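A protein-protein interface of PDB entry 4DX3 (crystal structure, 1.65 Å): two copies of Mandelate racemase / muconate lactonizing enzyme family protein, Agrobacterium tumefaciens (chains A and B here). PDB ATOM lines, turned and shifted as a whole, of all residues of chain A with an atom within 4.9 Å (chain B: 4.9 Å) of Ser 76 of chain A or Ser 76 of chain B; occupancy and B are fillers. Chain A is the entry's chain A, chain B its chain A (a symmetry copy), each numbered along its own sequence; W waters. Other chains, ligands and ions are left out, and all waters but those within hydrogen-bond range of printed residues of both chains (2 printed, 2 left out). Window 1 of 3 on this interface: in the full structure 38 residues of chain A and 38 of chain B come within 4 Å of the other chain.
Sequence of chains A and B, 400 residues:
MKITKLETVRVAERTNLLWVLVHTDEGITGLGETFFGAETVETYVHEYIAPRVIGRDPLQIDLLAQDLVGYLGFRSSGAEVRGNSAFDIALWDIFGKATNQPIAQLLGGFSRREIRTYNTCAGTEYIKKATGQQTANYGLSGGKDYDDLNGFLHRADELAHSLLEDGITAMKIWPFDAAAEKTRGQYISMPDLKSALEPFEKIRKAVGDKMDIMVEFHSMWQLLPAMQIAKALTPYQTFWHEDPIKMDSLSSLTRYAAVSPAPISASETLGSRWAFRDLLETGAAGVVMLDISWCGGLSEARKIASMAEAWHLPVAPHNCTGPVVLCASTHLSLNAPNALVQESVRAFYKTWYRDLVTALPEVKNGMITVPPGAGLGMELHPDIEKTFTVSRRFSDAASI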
ATOM      1  N   GLY A  73      -1.789 -21.250 -14.960  1.00  0.00           N
ATOM      2  CA  GLY A  73      -1.138 -20.427 -13.945  1.00  0.00           C
ATOM      3  C   GLY A  73      -1.453 -18.945 -13.996  1.00  0.00           C
ATOM      4  O   GLY A  73      -0.842 -18.141 -13.282  1.00  0.00           O
ATOM      5  N   PHE A  74      -2.413 -18.578 -14.834  1.00  0.00           N
ATOM      6  CA  PHE A  74      -2.832 -17.189 -14.948  1.00  0.00           C
ATOM      7  C   PHE A  74      -3.771 -16.830 -13.801  1.00  0.00           C
ATOM      8  O   PHE A  74      -4.218 -17.702 -13.050  1.00  0.00           O
ATOM      9  CB  PHE A  74      -3.552 -16.985 -16.291  1.00  0.00           C
ATOM     10  CG  PHE A  74      -4.721 -17.912 -16.475  1.00  0.00           C
ATOM     11  CD1 PHE A  74      -4.542 -19.180 -17.020  1.00  0.00           C
ATOM     12  CD2 PHE A  74      -5.992 -17.531 -16.062  1.00  0.00           C
ATOM     13  CE1 PHE A  74      -5.616 -20.045 -17.161  1.00  0.00           C
ATOM     14  CE2 PHE A  74      -7.073 -18.393 -16.197  1.00  0.00           C
ATOM     15  CZ  PHE A  74      -6.880 -19.657 -16.750  1.00  0.00           C
ATOM     16  N   ARG A  75      -4.081 -15.538 -13.696  1.00  0.00           N
ATOM     17  CA  ARG A  75      -4.981 -15.020 -12.660  1.00  0.00           C
ATOM     18  C   ARG A  75      -4.610 -15.601 -11.291  1.00  0.00           C
ATOM     19  O   ARG A  75      -5.455 -16.132 -10.547  1.00  0.00           O
ATOM     20  CB  ARG A  75      -6.438 -15.342 -13.012  1.00  0.00           C
ATOM     21  CG  ARG A  75      -7.467 -14.595 -12.157  1.00  0.00           C
ATOM     22  CD  ARG A  75      -8.565 -15.574 -11.759  1.00  0.00           C
ATOM     23  NE  ARG A  75      -9.633 -14.959 -10.965  1.00  0.00           N
ATOM     24  CZ  ARG A  75      -9.694 -15.004  -9.635  1.00  0.00           C
ATOM     25  NH1 ARG A  75      -8.745 -15.619  -8.940  1.00  0.00           N
ATOM     26  NH2 ARG A  75     -10.711 -14.425  -9.000  1.00  0.00           N
ATOM     27  N   SER A  76      -3.334 -15.496 -10.960  1.00  0.00           N
ATOM     28  CA  SER A  76      -2.845 -16.066  -9.720  1.00  0.00           C
ATOM     29  C   SER A  76      -1.594 -15.327  -9.315  1.00  0.00           C
ATOM     30  O   SER A  76      -1.097 -14.483 -10.060  1.00  0.00           O
ATOM     31  CB  SER A  76      -2.537 -17.547  -9.905  1.00  0.00           C
ATOM     32  OG  SER A  76      -1.262 -17.735 -10.482  1.00  0.00           O
ATOM     33  N   SER A  77      -1.081 -15.664  -8.140  1.00  0.00           N
ATOM     34  CA  SER A  77       0.184 -15.110  -7.674  1.00  0.00           C
ATOM     35  C   SER A  77       1.250 -16.201  -7.654  1.00  0.00           C
ATOM     36  O   SER A  77       2.192 -16.149  -6.846  1.00  0.00           O
ATOM     37  CB  SER A  77       0.014 -14.495  -6.290  1.00  0.00           C
ATOM     38  OG  SER A  77      -0.734 -15.351  -5.444  1.00  0.00           O
ATOM     39  N   GLY A  78       1.099 -17.178  -8.556  1.00  0.00           N
ATOM     40  CA  GLY A  78       1.985 -18.332  -8.616  1.00  0.00           C
ATOM     41  C   GLY A  78       3.327 -17.995  -9.234  1.00  0.00           C
ATOM     42  O   GLY A  78       3.556 -16.849  -9.614  1.00  0.00           O
ATOM     43  N   VAL A  81       3.591 -16.091 -12.599  1.00  0.00           N
ATOM     44  CA  VAL A  81       3.196 -14.692 -12.519  1.00  0.00           C
ATOM     45  C   VAL A  81       4.244 -13.859 -11.787  1.00  0.00           C
ATOM     46  O   VAL A  81       4.524 -12.722 -12.177  1.00  0.00           O
ATOM     47  CB  VAL A  81       1.827 -14.556 -11.862  1.00  0.00           C
ATOM     48  CG1 VAL A  81       1.507 -13.088 -11.548  1.00  0.00           C
ATOM     49  CG2 VAL A  81       0.775 -15.172 -12.793  1.00  0.00           C
ATOM     50  N   GLY A 271      -3.851 -12.053  -8.300  1.00  0.00           N
ATOM     51  CA  GLY A 271      -3.117 -11.663  -9.495  1.00  0.00           C
ATOM     52  C   GLY A 271      -3.974 -11.348 -10.711  1.00  0.00           C
ATOM     53  O   GLY A 271      -4.978 -12.023 -10.972  1.00  0.00           O
ATOM     54  N   TRP A 294       3.733  -9.667  -7.496  1.00  0.00           N
ATOM     55  CA  TRP A 294       2.889 -10.858  -7.375  1.00  0.00           C
ATOM     56  C   TRP A 294       1.651 -10.793  -8.273  1.00  0.00           C
ATOM     57  O   TRP A 294       0.948 -11.794  -8.426  1.00  0.00           O
ATOM     58  CB  TRP A 294       2.425 -11.050  -5.918  1.00  0.00           C
ATOM     59  CG  TRP A 294       3.529 -11.313  -4.923  1.00  0.00           C
ATOM     60  CD1 TRP A 294       4.824 -11.644  -5.200  1.00  0.00           C
ATOM     61  CD2 TRP A 294       3.429 -11.233  -3.495  1.00  0.00           C
ATOM     62  NE1 TRP A 294       5.538 -11.791  -4.025  1.00  0.00           N
ATOM     63  CE2 TRP A 294       4.707 -11.539  -2.966  1.00  0.00           C
ATOM     64  CE3 TRP A 294       2.386 -10.934  -2.608  1.00  0.00           C
ATOM     65  CZ2 TRP A 294       4.964 -11.561  -1.590  1.00  0.00           C
ATOM     66  CZ3 TRP A 294       2.644 -10.960  -1.242  1.00  0.00           C
ATOM     67  CH2 TRP A 294       3.922 -11.266  -0.749  1.00  0.00           C
ATOM     68  N   GLY B  73      -0.270 -18.374  -5.138  1.00  0.00           N
ATOM     69  CA  GLY B  73      -0.323 -19.384  -6.190  1.00  0.00           C
ATOM     70  C   GLY B  73      -1.416 -20.425  -6.050  1.00  0.00           C
ATOM     71  O   GLY B  73      -1.456 -21.408  -6.800  1.00  0.00           O
ATOM     72  N   PHE B  74      -2.310 -20.212  -5.096  1.00  0.00           N
ATOM     73  CA  PHE B  74      -3.428 -21.120  -4.885  1.00  0.00           C
ATOM     74  C   PHE B  74      -4.528 -20.841  -5.904  1.00  0.00           C
ATOM     75  O   PHE B  74      -4.483 -19.843  -6.629  1.00  0.00           O
ATOM     76  CB  PHE B  74      -3.977 -20.926  -3.462  1.00  0.00           C
ATOM     77  CG  PHE B  74      -4.382 -19.507  -3.179  1.00  0.00           C
ATOM     78  CD1 PHE B  74      -3.453 -18.586  -2.704  1.00  0.00           C
ATOM     79  CD2 PHE B  74      -5.682 -19.084  -3.430  1.00  0.00           C
ATOM     80  CE1 PHE B  74      -3.821 -17.269  -2.472  1.00  0.00           C
ATOM     81  CE2 PHE B  74      -6.058 -17.766  -3.203  1.00  0.00           C
ATOM     82  CZ  PHE B  74      -5.119 -16.856  -2.721  1.00  0.00           C
ATOM     83  N   ARG B  75      -5.526 -21.723  -5.926  1.00  0.00           N
ATOM     84  CA  ARG B  75      -6.673 -21.601  -6.833  1.00  0.00           C
ATOM     85  C   ARG B  75      -6.197 -21.285  -8.256  1.00  0.00           C
ATOM     86  O   ARG B  75      -6.669 -20.341  -8.916  1.00  0.00           O
ATOM     87  CB  ARG B  75      -7.637 -20.521  -6.328  1.00  0.00           C
ATOM     88  CG  ARG B  75      -8.998 -20.520  -7.032  1.00  0.00           C
ATOM     89  CD  ARG B  75      -9.383 -19.078  -7.337  1.00  0.00           C
ATOM     90  NE  ARG B  75     -10.693 -18.948  -7.981  1.00  0.00           N
ATOM     91  CZ  ARG B  75     -10.870 -18.830  -9.296  1.00  0.00           C
ATOM     92  NH1 ARG B  75      -9.826 -18.838 -10.117  1.00  0.00           N
ATOM     93  NH2 ARG B  75     -12.100 -18.705  -9.790  1.00  0.00           N
ATOM     94  N   SER B  76      -5.254 -22.084  -8.726  1.00  0.00           N
ATOM     95  CA  SER B  76      -4.674 -21.849 -10.034  1.00  0.00           C
ATOM     96  C   SER B  76      -4.121 -23.152 -10.552  1.00  0.00           C
ATOM     97  O   SER B  76      -4.110 -24.156  -9.839  1.00  0.00           O
ATOM     98  CB  SER B  76      -3.560 -20.812  -9.938  1.00  0.00           C
ATOM     99  OG  SER B  76      -2.348 -21.403  -9.518  1.00  0.00           O
ATOM    100  N   SER B  77      -3.646 -23.125 -11.790  1.00  0.00           N
ATOM    101  CA  SER B  77      -2.983 -24.282 -12.377  1.00  0.00           C
ATOM    102  C   SER B  77      -1.497 -23.990 -12.558  1.00  0.00           C
ATOM    103  O   SER B  77      -0.851 -24.539 -13.466  1.00  0.00           O
ATOM    104  CB  SER B  77      -3.628 -24.642 -13.710  1.00  0.00           C
ATOM    105  OG  SER B  77      -3.850 -23.483 -14.495  1.00  0.00           O
ATOM    106  N   GLY B  78      -0.961 -23.133 -11.681  1.00  0.00           N
ATOM    107  CA  GLY B  78       0.423 -22.689 -11.763  1.00  0.00           C
ATOM    108  C   GLY B  78       1.396 -23.751 -11.291  1.00  0.00           C
ATOM    109  O   GLY B  78       0.975 -24.837 -10.899  1.00  0.00           O
ATOM    110  N   VAL B  81       0.916 -25.587  -7.913  1.00  0.00           N
ATOM    111  CA  VAL B  81      -0.211 -26.510  -7.897  1.00  0.00           C
ATOM    112  C   VAL B  81       0.087 -27.764  -8.713  1.00  0.00           C
ATOM    113  O   VAL B  81      -0.286 -28.872  -8.318  1.00  0.00           O
ATOM    114  CB  VAL B  81      -1.479 -25.820  -8.388  1.00  0.00           C
ATOM    115  CG1 VAL B  81      -2.609 -26.835  -8.610  1.00  0.00           C
ATOM    116  CG2 VAL B  81      -1.880 -24.750  -7.365  1.00  0.00           C
ATOM    117  N   GLY B 271      -7.936 -24.527 -11.184  1.00  0.00           N
ATOM    118  CA  GLY B 271      -7.422 -25.307 -10.069  1.00  0.00           C
ATOM    119  C   GLY B 271      -8.161 -25.122  -8.751  1.00  0.00           C
ATOM    120  O   GLY B 271      -8.566 -24.007  -8.402  1.00  0.00           O
ATOM    121  N   TRP B 294      -3.202 -30.767 -12.765  1.00  0.00           N
ATOM    122  CA  TRP B 294      -3.227 -29.304 -12.831  1.00  0.00           C
ATOM    123  C   TRP B 294      -4.170 -28.687 -11.796  1.00  0.00           C
ATOM    124  O   TRP B 294      -4.158 -27.469 -11.600  1.00  0.00           O
ATOM    125  CB  TRP B 294      -3.663 -28.830 -14.231  1.00  0.00           C
ATOM    126  CG  TRP B 294      -2.727 -29.206 -15.355  1.00  0.00           C
ATOM    127  CD1 TRP B 294      -1.452 -29.678 -15.240  1.00  0.00           C
ATOM    128  CD2 TRP B 294      -3.018 -29.164 -16.759  1.00  0.00           C
ATOM    129  NE1 TRP B 294      -0.921 -29.921 -16.494  1.00  0.00           N
ATOM    130  CE2 TRP B 294      -1.863 -29.619 -17.441  1.00  0.00           C
ATOM    131  CE3 TRP B 294      -4.139 -28.785 -17.509  1.00  0.00           C
ATOM    132  CZ2 TRP B 294      -1.798 -29.697 -18.838  1.00  0.00           C
ATOM    133  CZ3 TRP B 294      -4.070 -28.861 -18.896  1.00  0.00           C
ATOM    134  CH2 TRP B 294      -2.912 -29.318 -19.543  1.00  0.00           C
HETATM  135  O   HOH W   1      -4.347 -20.458 -13.157  1.00  0.00           O
HETATM  136  O   HOH W   2      -3.011 -17.507  -6.607  1.00  0.00           O
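Gly 73 of chain A touches Ser 77 of chain B, and with the chains exchanged Ser 77 of chain A touches Gly 73 of chain B. Gly 73 of chain A touches Gly 78 of chain B, and with the chains exchanged Gly 78 of chain A touches Gly 73 of chain B. Arg 75 of chain B touches its own counterpart, Arg 75 of chain A. Ser 76 of chain B touches its own counterpart, Ser 76 of chain A. Positions printed for both chains: 73, 74, 75, 76, 77, 78, 81, 271 and 294.
Water W1 lies within hydrogen-bond range of O of Phe 74 of chain A (2.8 Å), N of Ser 77 of chain B (3.1 Å) and N of Gly 73 of chain A (3.2 Å). Water W2 lies within hydrogen-bond range of O of Phe 74 of chain B (2.8 Å), N of Ser 77 of chain A (3.1 Å) and N of Gly 73 of chain B (3.2 Å).
Of chain A, only Ser 76 comes within 4 Å of Ser 76 of chain B. Printed residues of chain A within 4 Å of Ser 77 of chain B: Gly 73. Of the printed residues of chain B, Gly 73 of chain A touches Ser 77 and Gly 78. Of the printed residues of chain B, Ser 77 of chain A touches Gly 73. Phe 74 of chain A touches none of the printed residues of chain B. The nearest residue of chain B that does not touch Ser 76 of chain A is Phe 74 of chain B (4.4 Å). The nearest residue of chain A that does not touch Ser 76 of chain B is Phe 74 of chain A (4.4 Å).
N of Gly 73 of chain A is in hydrogen-bond range of OG of Ser 77 of chain B (3.1 Å). The side-chain hydroxyl (OG) of Ser 77 of chain A is in hydrogen-bond range of the backbone NH (N) of Gly 73 of chain B (3.1 Å).
Among the printed residues, pairs that only touch across the chains: Ser 76 of chain A with Ser 76 of chain B (3.4 Å), Gly 73 of chain A with Gly 78 of chain B (3.5 Å), Gly 78 of chain A with Gly 73 of chain B (3.5 Å) and Arg 75 of chain A with Arg 75 of chain B (3.6 Å).
Printed residues of chain A that touch a printed residue of chain B: Gly 73, Arg 75, Ser 76, Ser 77 and Gly 78. Among the printed residues, no Asp or Glu carboxylate lies within 4 Å of a Lys or Arg side-chain nitrogen of the other chain.
The backbone carbonyl oxygen (O) of Gly 73 of chain A sits at hydrogen-bond distance from the side-chain hydroxyl (OG) of Ser 76 of chain A (2.9 Å). The side-chain hydroxyl (OG) of Ser 76 of chain A sits at hydrogen-bond distance from the backbone NH (N) of Gly 78 of chain A. The backbone carbonyl oxygen (O) of Gly 73 of chain B is in hydrogen-bond range of the side-chain hydroxyl (OG) of Ser 76 of chain B, at 2.9 Å. The backbone NH (N) of Gly 78 of chain B is in hydrogen-bond range of the side-chain hydroxyl (OG) of Ser 76 of chain B (3.1 Å).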
